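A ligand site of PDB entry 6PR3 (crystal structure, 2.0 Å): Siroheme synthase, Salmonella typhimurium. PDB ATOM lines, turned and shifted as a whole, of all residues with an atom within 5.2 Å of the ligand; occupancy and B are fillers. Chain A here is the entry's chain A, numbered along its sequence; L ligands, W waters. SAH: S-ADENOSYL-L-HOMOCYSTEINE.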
ATOM      1  N   PRO A 225       9.418  -6.535  -9.399  1.00  0.00           N
ATOM      2  CA  PRO A 225       9.045  -5.475 -10.354  1.00  0.00           C
ATOM      3  C   PRO A 225       8.226  -5.943 -11.543  1.00  0.00           C
ATOM      4  O   PRO A 225       7.739  -5.104 -12.320  1.00  0.00           O
ATOM      5  CB  PRO A 225      10.406  -4.908 -10.784  1.00  0.00           C
ATOM      6  CG  PRO A 225      11.380  -6.036 -10.585  1.00  0.00           C
ATOM      7  CD  PRO A 225      10.817  -6.983  -9.562  1.00  0.00           C
ATOM      8  N   GLY A 226       8.043  -7.243 -11.709  1.00  0.00           N
ATOM      9  CA  GLY A 226       7.117  -7.702 -12.743  1.00  0.00           C
ATOM     10  C   GLY A 226       7.318  -9.150 -13.172  1.00  0.00           C
ATOM     11  O   GLY A 226       6.354  -9.929 -13.195  1.00  0.00           O
ATOM     12  N   LEU A 250       0.709  -2.131  -9.743  1.00  0.00           N
ATOM     13  CA  LEU A 250       2.125  -2.419  -9.952  1.00  0.00           C
ATOM     14  C   LEU A 250       2.476  -3.867  -9.692  1.00  0.00           C
ATOM     15  O   LEU A 250       3.666  -4.228  -9.724  1.00  0.00           O
ATOM     16  CB  LEU A 250       2.973  -1.488  -9.083  1.00  0.00           C
ATOM     17  CG  LEU A 250       2.797  -0.002  -9.421  1.00  0.00           C
ATOM     18  CD1 LEU A 250       3.557   0.870  -8.448  1.00  0.00           C
ATOM     19  CD2 LEU A 250       3.225   0.279 -10.859  1.00  0.00           C
ATOM     20  N   GLY A 301       3.975  -4.136  -5.401  1.00  0.00           N
ATOM     21  CA  GLY A 301       5.033  -4.113  -6.400  1.00  0.00           C
ATOM     22  C   GLY A 301       6.397  -3.903  -5.748  1.00  0.00           C
ATOM     23  O   GLY A 301       6.520  -3.185  -4.744  1.00  0.00           O
ATOM     24  N   GLY A 302       7.409  -4.552  -6.308  1.00  0.00           N
ATOM     25  CA  GLY A 302       8.772  -4.362  -5.841  1.00  0.00           C
ATOM     26  C   GLY A 302       8.971  -4.862  -4.425  1.00  0.00           C
ATOM     27  O   GLY A 302       8.596  -5.993  -4.078  1.00  0.00           O
ATOM     28  N   ASP A 303       9.544  -4.011  -3.577  1.00  0.00           N
ATOM     29  CA  ASP A 303       9.794  -4.272  -2.166  1.00  0.00           C
ATOM     30  C   ASP A 303       8.823  -3.467  -1.295  1.00  0.00           C
ATOM     31  O   ASP A 303       8.602  -2.291  -1.562  1.00  0.00           O
ATOM     32  CB  ASP A 303      11.239  -3.904  -1.787  1.00  0.00           C
ATOM     33  CG  ASP A 303      11.572  -4.254  -0.327  1.00  0.00           C
ATOM     34  OD1 ASP A 303      11.724  -5.456  -0.012  1.00  0.00           O
ATOM     35  OD2 ASP A 303      11.633  -3.323   0.520  1.00  0.00           O
ATOM     36  N   PRO A 304       8.259  -4.078  -0.240  1.00  0.00           N
ATOM     37  CA  PRO A 304       7.191  -3.402   0.535  1.00  0.00           C
ATOM     38  C   PRO A 304       7.664  -2.207   1.339  1.00  0.00           C
ATOM     39  O   PRO A 304       6.836  -1.360   1.687  1.00  0.00           O
ATOM     40  CB  PRO A 304       6.661  -4.504   1.464  1.00  0.00           C
ATOM     41  CG  PRO A 304       7.177  -5.777   0.910  1.00  0.00           C
ATOM     42  CD  PRO A 304       8.455  -5.473   0.201  1.00  0.00           C
ATOM     43  N   ILE A 306      10.259  -0.025   0.496  1.00  0.00           N
ATOM     44  CA  ILE A 306      10.913   0.995  -0.314  1.00  0.00           C
ATOM     45  C   ILE A 306       9.823   1.748  -1.075  1.00  0.00           C
ATOM     46  O   ILE A 306       9.303   1.257  -2.096  1.00  0.00           O
ATOM     47  CB  ILE A 306      11.963   0.392  -1.267  1.00  0.00           C
ATOM     48  CG1 ILE A 306      13.121  -0.173  -0.423  1.00  0.00           C
ATOM     49  CG2 ILE A 306      12.453   1.454  -2.293  1.00  0.00           C
ATOM     50  CD1 ILE A 306      14.241  -0.838  -1.207  1.00  0.00           C
ATOM     51  N   PHE A 307       9.458   2.925  -0.567  1.00  0.00           N
ATOM     52  CA  PHE A 307       8.406   3.771  -1.163  1.00  0.00           C
ATOM     53  C   PHE A 307       7.106   2.997  -1.375  1.00  0.00           C
ATOM     54  O   PHE A 307       6.373   3.241  -2.335  1.00  0.00           O
ATOM     55  CB  PHE A 307       8.890   4.387  -2.471  1.00  0.00           C
ATOM     56  CG  PHE A 307      10.149   5.212  -2.333  1.00  0.00           C
ATOM     57  CD1 PHE A 307      10.181   6.315  -1.485  1.00  0.00           C
ATOM     58  CD2 PHE A 307      11.301   4.869  -3.028  1.00  0.00           C
ATOM     59  CE1 PHE A 307      11.349   7.078  -1.347  1.00  0.00           C
ATOM     60  CE2 PHE A 307      12.460   5.609  -2.891  1.00  0.00           C
ATOM     61  CZ  PHE A 307      12.486   6.724  -2.055  1.00  0.00           C
ATOM     62  N   GLY A 308       6.806   2.074  -0.477  1.00  0.00           N
ATOM     63  CA  GLY A 308       5.589   1.295  -0.628  1.00  0.00           C
ATOM     64  C   GLY A 308       4.453   1.625   0.324  1.00  0.00           C
ATOM     65  O   GLY A 308       3.356   1.080   0.176  1.00  0.00           O
ATOM     66  N   ILE A 330      12.204  -7.986  -4.632  1.00  0.00           N
ATOM     67  CA  ILE A 330      13.172  -7.290  -5.481  1.00  0.00           C
ATOM     68  C   ILE A 330      12.629  -5.904  -5.790  1.00  0.00           C
ATOM     69  O   ILE A 330      11.609  -5.777  -6.478  1.00  0.00           O
ATOM     70  CB  ILE A 330      13.397  -8.067  -6.788  1.00  0.00           C
ATOM     71  CG1 ILE A 330      13.771  -9.529  -6.501  1.00  0.00           C
ATOM     72  CG2 ILE A 330      14.395  -7.299  -7.686  1.00  0.00           C
ATOM     73  CD1 ILE A 330      15.091  -9.678  -5.801  1.00  0.00           C
ATOM     74  N   THR A 331      13.318  -4.863  -5.315  1.00  0.00           N
ATOM     75  CA  THR A 331      12.830  -3.512  -5.611  1.00  0.00           C
ATOM     76  C   THR A 331      13.030  -3.158  -7.094  1.00  0.00           C
ATOM     77  O   THR A 331      13.788  -3.809  -7.829  1.00  0.00           O
ATOM     78  CB  THR A 331      13.483  -2.478  -4.672  1.00  0.00           C
ATOM     79  OG1 THR A 331      12.833  -1.189  -4.808  1.00  0.00           O
ATOM     80  CG2 THR A 331      14.994  -2.334  -4.956  1.00  0.00           C
ATOM     81  N   ALA A 332      12.302  -2.142  -7.557  1.00  0.00           N
ATOM     82  CA  ALA A 332      12.415  -1.791  -8.978  1.00  0.00           C
ATOM     83  C   ALA A 332      13.873  -1.501  -9.358  1.00  0.00           C
ATOM     84  O   ALA A 332      14.319  -1.875 -10.447  1.00  0.00           O
ATOM     85  CB  ALA A 332      11.505  -0.595  -9.294  1.00  0.00           C
ATOM     86  N   ALA A 333      14.631  -0.842  -8.453  1.00  0.00           N
ATOM     87  CA  ALA A 333      16.016  -0.489  -8.749  1.00  0.00           C
ATOM     88  C   ALA A 333      16.853  -1.723  -9.071  1.00  0.00           C
ATOM     89  O   ALA A 333      17.585  -1.752 -10.069  1.00  0.00           O
ATOM     90  CB  ALA A 333      16.653   0.261  -7.574  1.00  0.00           C
ATOM     91  N   CYS A 336      15.443  -3.519 -12.447  1.00  0.00           N
ATOM     92  CA  CYS A 336      15.756  -2.790 -13.688  1.00  0.00           C
ATOM     93  C   CYS A 336      17.261  -2.719 -13.936  1.00  0.00           C
ATOM     94  O   CYS A 336      17.697  -2.709 -15.096  1.00  0.00           O
ATOM     95  CB  CYS A 336      15.180  -1.373 -13.655  1.00  0.00           C
ATOM     96  SG  CYS A 336      13.371  -1.267 -13.630  1.00  0.00           S
ATOM     97  N   PHE A 380      15.496   7.409  -9.443  1.00  0.00           N
ATOM     98  CA  PHE A 380      14.290   8.158  -9.110  1.00  0.00           C
ATOM     99  C   PHE A 380      13.094   7.258  -9.322  1.00  0.00           C
ATOM    100  O   PHE A 380      12.889   6.728 -10.418  1.00  0.00           O
ATOM    101  CB  PHE A 380      14.152   9.412  -9.973  1.00  0.00           C
ATOM    102  CG  PHE A 380      15.149  10.473  -9.658  1.00  0.00           C
ATOM    103  CD1 PHE A 380      14.874  11.438  -8.687  1.00  0.00           C
ATOM    104  CD2 PHE A 380      16.384  10.479 -10.278  1.00  0.00           C
ATOM    105  CE1 PHE A 380      15.798  12.401  -8.385  1.00  0.00           C
ATOM    106  CE2 PHE A 380      17.319  11.437  -9.968  1.00  0.00           C
ATOM    107  CZ  PHE A 380      17.035  12.397  -9.014  1.00  0.00           C
ATOM    108  N   TYR A 381      12.324   7.087  -8.255  1.00  0.00           N
ATOM    109  CA  TYR A 381      11.025   6.430  -8.312  1.00  0.00           C
ATOM    110  C   TYR A 381       9.947   7.492  -8.491  1.00  0.00           C
ATOM    111  O   TYR A 381      10.056   8.603  -7.964  1.00  0.00           O
ATOM    112  CB  TYR A 381      10.759   5.674  -7.017  1.00  0.00           C
ATOM    113  CG  TYR A 381      11.587   4.414  -6.814  1.00  0.00           C
ATOM    114  CD1 TYR A 381      12.953   4.472  -6.536  1.00  0.00           C
ATOM    115  CD2 TYR A 381      10.974   3.153  -6.850  1.00  0.00           C
ATOM    116  CE1 TYR A 381      13.699   3.299  -6.322  1.00  0.00           C
ATOM    117  CE2 TYR A 381      11.700   1.987  -6.628  1.00  0.00           C
ATOM    118  CZ  TYR A 381      13.055   2.055  -6.370  1.00  0.00           C
ATOM    119  OH  TYR A 381      13.747   0.889  -6.164  1.00  0.00           O
ATOM    120  N   MET A 382       8.905   7.127  -9.247  1.00  0.00           N
ATOM    121  CA  MET A 382       7.789   8.022  -9.629  1.00  0.00           C
ATOM    122  C   MET A 382       8.251   9.442  -9.934  1.00  0.00           C
ATOM    123  O   MET A 382       7.745  10.428  -9.396  1.00  0.00           O
ATOM    124  CB  MET A 382       6.679   8.005  -8.578  1.00  0.00           C
ATOM    125  CG  MET A 382       7.085   8.331  -7.168  1.00  0.00           C
ATOM    126  SD  MET A 382       6.142   7.416  -5.912  1.00  0.00           S
ATOM    127  CE  MET A 382       7.431   7.218  -4.680  1.00  0.00           C
ATOM    128  N   GLY A 383       9.226   9.543 -10.837  1.00  0.00           N
ATOM    129  CA  GLY A 383       9.753  10.853 -11.182  1.00  0.00           C
ATOM    130  C   GLY A 383       9.482  11.284 -12.607  1.00  0.00           C
ATOM    131  O   GLY A 383       9.977  12.317 -13.055  1.00  0.00           O
ATOM    132  N   VAL A 408      13.935   3.196 -17.621  1.00  0.00           N
ATOM    133  CA  VAL A 408      13.525   1.807 -17.809  1.00  0.00           C
ATOM    134  C   VAL A 408      12.029   1.737 -17.531  1.00  0.00           C
ATOM    135  O   VAL A 408      11.592   1.981 -16.409  1.00  0.00           O
ATOM    136  CB  VAL A 408      14.309   0.850 -16.895  1.00  0.00           C
ATOM    137  CG1 VAL A 408      13.891  -0.639 -17.167  1.00  0.00           C
ATOM    138  CG2 VAL A 408      15.792   1.074 -17.102  1.00  0.00           C
ATOM    139  N   GLU A 409      11.241   1.430 -18.571  1.00  0.00           N
ATOM    140  CA  GLU A 409       9.805   1.264 -18.455  1.00  0.00           C
ATOM    141  C   GLU A 409       9.453  -0.227 -18.384  1.00  0.00           C
ATOM    142  O   GLU A 409       9.982  -1.023 -19.158  1.00  0.00           O
ATOM    143  CB  GLU A 409       9.083   1.912 -19.636  1.00  0.00           C
ATOM    144  CG  GLU A 409       7.590   1.641 -19.659  1.00  0.00           C
ATOM    145  CD  GLU A 409       6.862   2.413 -20.741  1.00  0.00           C
ATOM    146  OE1 GLU A 409       7.522   2.925 -21.667  1.00  0.00           O
ATOM    147  OE2 GLU A 409       5.618   2.493 -20.666  1.00  0.00           O
ATOM    148  N   ASN A 410       8.561  -0.582 -17.454  1.00  0.00           N
ATOM    149  CA  ASN A 410       8.117  -1.960 -17.292  1.00  0.00           C
ATOM    150  C   ASN A 410       9.315  -2.906 -17.205  1.00  0.00           C
ATOM    151  O   ASN A 410       9.382  -3.925 -17.896  1.00  0.00           O
ATOM    152  CB  ASN A 410       7.169  -2.367 -18.436  1.00  0.00           C
ATOM    153  CG  ASN A 410       5.790  -1.756 -18.273  1.00  0.00           C
ATOM    154  OD1 ASN A 410       5.184  -1.880 -17.207  1.00  0.00           O
ATOM    155  ND2 ASN A 410       5.288  -1.088 -19.312  1.00  0.00           N
ATOM    156  N   GLY A 411      10.255  -2.547 -16.328  1.00  0.00           N
ATOM    157  CA  GLY A 411      11.486  -3.313 -16.205  1.00  0.00           C
ATOM    158  C   GLY A 411      11.206  -4.738 -15.754  1.00  0.00           C
ATOM    159  O   GLY A 411      10.327  -4.992 -14.933  1.00  0.00           O
ATOM    160  N   THR A 412      11.988  -5.670 -16.324  1.00  0.00           N
ATOM    161  CA  THR A 412      11.937  -7.127 -16.127  1.00  0.00           C
ATOM    162  C   THR A 412      10.736  -7.799 -16.808  1.00  0.00           C
ATOM    163  O   THR A 412      10.656  -9.038 -16.825  1.00  0.00           O
ATOM    164  CB  THR A 412      11.959  -7.534 -14.637  1.00  0.00           C
ATOM    165  OG1 THR A 412      10.651  -7.447 -14.050  1.00  0.00           O
ATOM    166  CG2 THR A 412      13.030  -6.718 -13.804  1.00  0.00           C
ATOM    167  N   PRO A 436       4.822   2.328 -15.449  1.00  0.00           N
ATOM    168  CA  PRO A 436       5.835   2.619 -14.428  1.00  0.00           C
ATOM    169  C   PRO A 436       7.228   2.713 -15.058  1.00  0.00           C
ATOM    170  O   PRO A 436       7.627   1.827 -15.814  1.00  0.00           O
ATOM    171  CB  PRO A 436       5.736   1.419 -13.469  1.00  0.00           C
ATOM    172  CG  PRO A 436       5.290   0.289 -14.355  1.00  0.00           C
ATOM    173  CD  PRO A 436       4.426   0.902 -15.456  1.00  0.00           C
ATOM    174  N   ALA A 437       7.950   3.792 -14.756  1.00  0.00           N
ATOM    175  CA  ALA A 437       9.308   3.929 -15.248  1.00  0.00           C
ATOM    176  C   ALA A 437      10.233   4.392 -14.131  1.00  0.00           C
ATOM    177  O   ALA A 437       9.831   5.113 -13.205  1.00  0.00           O
ATOM    178  CB  ALA A 437       9.396   4.908 -16.433  1.00  0.00           C
ATOM    179  N   LEU A 438      11.485   3.956 -14.236  1.00  0.00           N
ATOM    180  CA  LEU A 438      12.553   4.345 -13.323  1.00  0.00           C
ATOM    181  C   LEU A 438      13.510   5.250 -14.084  1.00  0.00           C
ATOM    182  O   LEU A 438      13.756   5.035 -15.271  1.00  0.00           O
ATOM    183  CB  LEU A 438      13.298   3.096 -12.837  1.00  0.00           C
ATOM    184  CG  LEU A 438      13.644   2.916 -11.374  1.00  0.00           C
ATOM    185  CD1 LEU A 438      12.406   3.054 -10.509  1.00  0.00           C
ATOM    186  CD2 LEU A 438      14.257   1.545 -11.229  1.00  0.00           C
HETATM  187  N   SAH L   1       7.837  -0.517  -3.634  1.00  0.00           N
HETATM  188  CA  SAH L   1       8.188  -0.426  -5.031  1.00  0.00           C
HETATM  189  CB  SAH L   1       8.096   1.018  -5.535  1.00  0.00           C
HETATM  190  CG  SAH L   1       6.687   1.618  -5.495  1.00  0.00           C
HETATM  191  SD  SAH L   1       6.739   3.399  -5.871  1.00  0.00           S
HETATM  192  C   SAH L   1       9.595  -0.990  -5.261  1.00  0.00           C
HETATM  193  O   SAH L   1      10.289  -1.406  -4.335  1.00  0.00           O
HETATM  194  OXT SAH L   1      10.067  -1.011  -6.385  1.00  0.00           O
HETATM  195  C5' SAH L   1       6.227   3.186  -7.598  1.00  0.00           C
HETATM  196  C4' SAH L   1       7.356   3.461  -8.582  1.00  0.00           C
HETATM  197  O4' SAH L   1       8.250   2.365  -8.680  1.00  0.00           O
HETATM  198  C3' SAH L   1       6.858   3.707 -10.000  1.00  0.00           C
HETATM  199  O3' SAH L   1       6.530   5.058 -10.185  1.00  0.00           O
HETATM  200  C2' SAH L   1       8.081   3.382 -10.813  1.00  0.00           C
HETATM  201  O2' SAH L   1       8.934   4.505 -10.767  1.00  0.00           O
HETATM  202  C1' SAH L   1       8.770   2.314  -9.990  1.00  0.00           C
HETATM  203  N9  SAH L   1       8.571   0.984 -10.568  1.00  0.00           N
HETATM  204  C8  SAH L   1       7.848  -0.061 -10.020  1.00  0.00           C
HETATM  205  N7  SAH L   1       7.918  -1.107 -10.861  1.00  0.00           N
HETATM  206  C5  SAH L   1       8.666  -0.766 -11.942  1.00  0.00           C
HETATM  207  C6  SAH L   1       9.042  -1.449 -13.102  1.00  0.00           C
HETATM  208  N6  SAH L   1       8.691  -2.720 -13.347  1.00  0.00           N
HETATM  209  N1  SAH L   1       9.810  -0.785 -14.028  1.00  0.00           N
HETATM  210  C2  SAH L   1      10.200   0.523 -13.828  1.00  0.00           C
HETATM  211  N3  SAH L   1       9.828   1.183 -12.676  1.00  0.00           N
HETATM  212  C4  SAH L   1       9.073   0.550 -11.755  1.00  0.00           C
HETATM  213  O   HOH W   1       3.877   4.567 -10.820  1.00  0.00           O
HETATM  214  O   HOH W   2       5.946  -1.033  -7.491  1.00  0.00           O
HETATM  215  O   HOH W   3       5.250  -1.093  -3.268  1.00  0.00           O
HETATM  216  O   HOH W   4       6.286  -3.188  -9.578  1.00  0.00           O
HETATM  217  O   HOH W   5       6.404   5.798 -13.132  1.00  0.00           O
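The side-chain hydroxyl (OG1) of Thr 331 lies within hydrogen-bond range of an oxygen (O) of the ligand (2.6 Å).
The backbone carbonyl oxygen (O) of Ala 437 lies within hydrogen-bond range of an oxygen (O2') of the ligand (2.7 Å).
The backbone carbonyl oxygen (O) of Pro 225 is in hydrogen-bond range of a nitrogen (N6) of the ligand, 2.8 Å away.
N of Ala 332 sits at hydrogen-bond distance from OXT of the ligand, at 2.8 Å.
O of Ile 306 is in hydrogen-bond range of N of the ligand (2.8 Å).
O of the ligand sits at hydrogen-bond distance from N of Asp 303 (2.8 Å).
A nitrogen (N) of the ligand sits at hydrogen-bond distance from the backbone carbonyl oxygen (O) of Asp 303 (2.8 Å).
The backbone NH of Gly 411 is in hydrogen-bond range of a nitrogen (N1) of the ligand, 2.9 Å away.
The backbone carbonyl oxygen (O) of Gly 411 lies within hydrogen-bond range of a nitrogen (N6) of the ligand (3.2 Å).
The backbone NH (N) of Met 382 is in hydrogen-bond range of an oxygen (O2') of the ligand (3.0 Å).
The backbone carbonyl oxygen (O) of Gly 301 is in hydrogen-bond range of a nitrogen (N) of the ligand (3.2 Å).
SG of Cys 336 sits at hydrogen-bond distance from N1 of the ligand (3.6 Å).
OG1 of Thr 331 sits at hydrogen-bond distance from OH of Tyr 381 (2.6 Å).
O of Ala 332 lies close to SG of Cys 336, at 3.4 Å.
N of Leu 438 sits at hydrogen-bond distance from O of Val 408, at 2.9 Å.
OH of Tyr 381 is in hydrogen-bond range of N of Ala 333.
O of Pro 436 is in hydrogen-bond range of N of Asn 410 (3.1 Å).
SD of the ligand sits close to O of Phe 307, 3.6 Å away.
Merely in contact with the ligand: Leu 250, Gly 302, Tyr 381, Val 408, Asn 410, Pro 436 and Leu 438.
Hydrophobic or aromatic side chains that line the ligand: Pro 225, Leu 250, Ile 306, Ala 332, Tyr 381, Met 382, Pro 436 and Leu 438.
The nearest printed residue that does not touch the ligand is Gly 308 (4.2 Å).
Water W3 lies within hydrogen-bond range of N of the ligand (2.7 Å) and O of Gly 301 (2.9 Å).
Water W4 lies within hydrogen-bond range of the backbone carbonyl oxygen (O) of Leu 250 and a nitrogen (N7) of the ligand.
Water W5 lies within hydrogen-bond range of N of Ala 437 (3.0 Å) and O3' of the ligand (3.0 Å).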
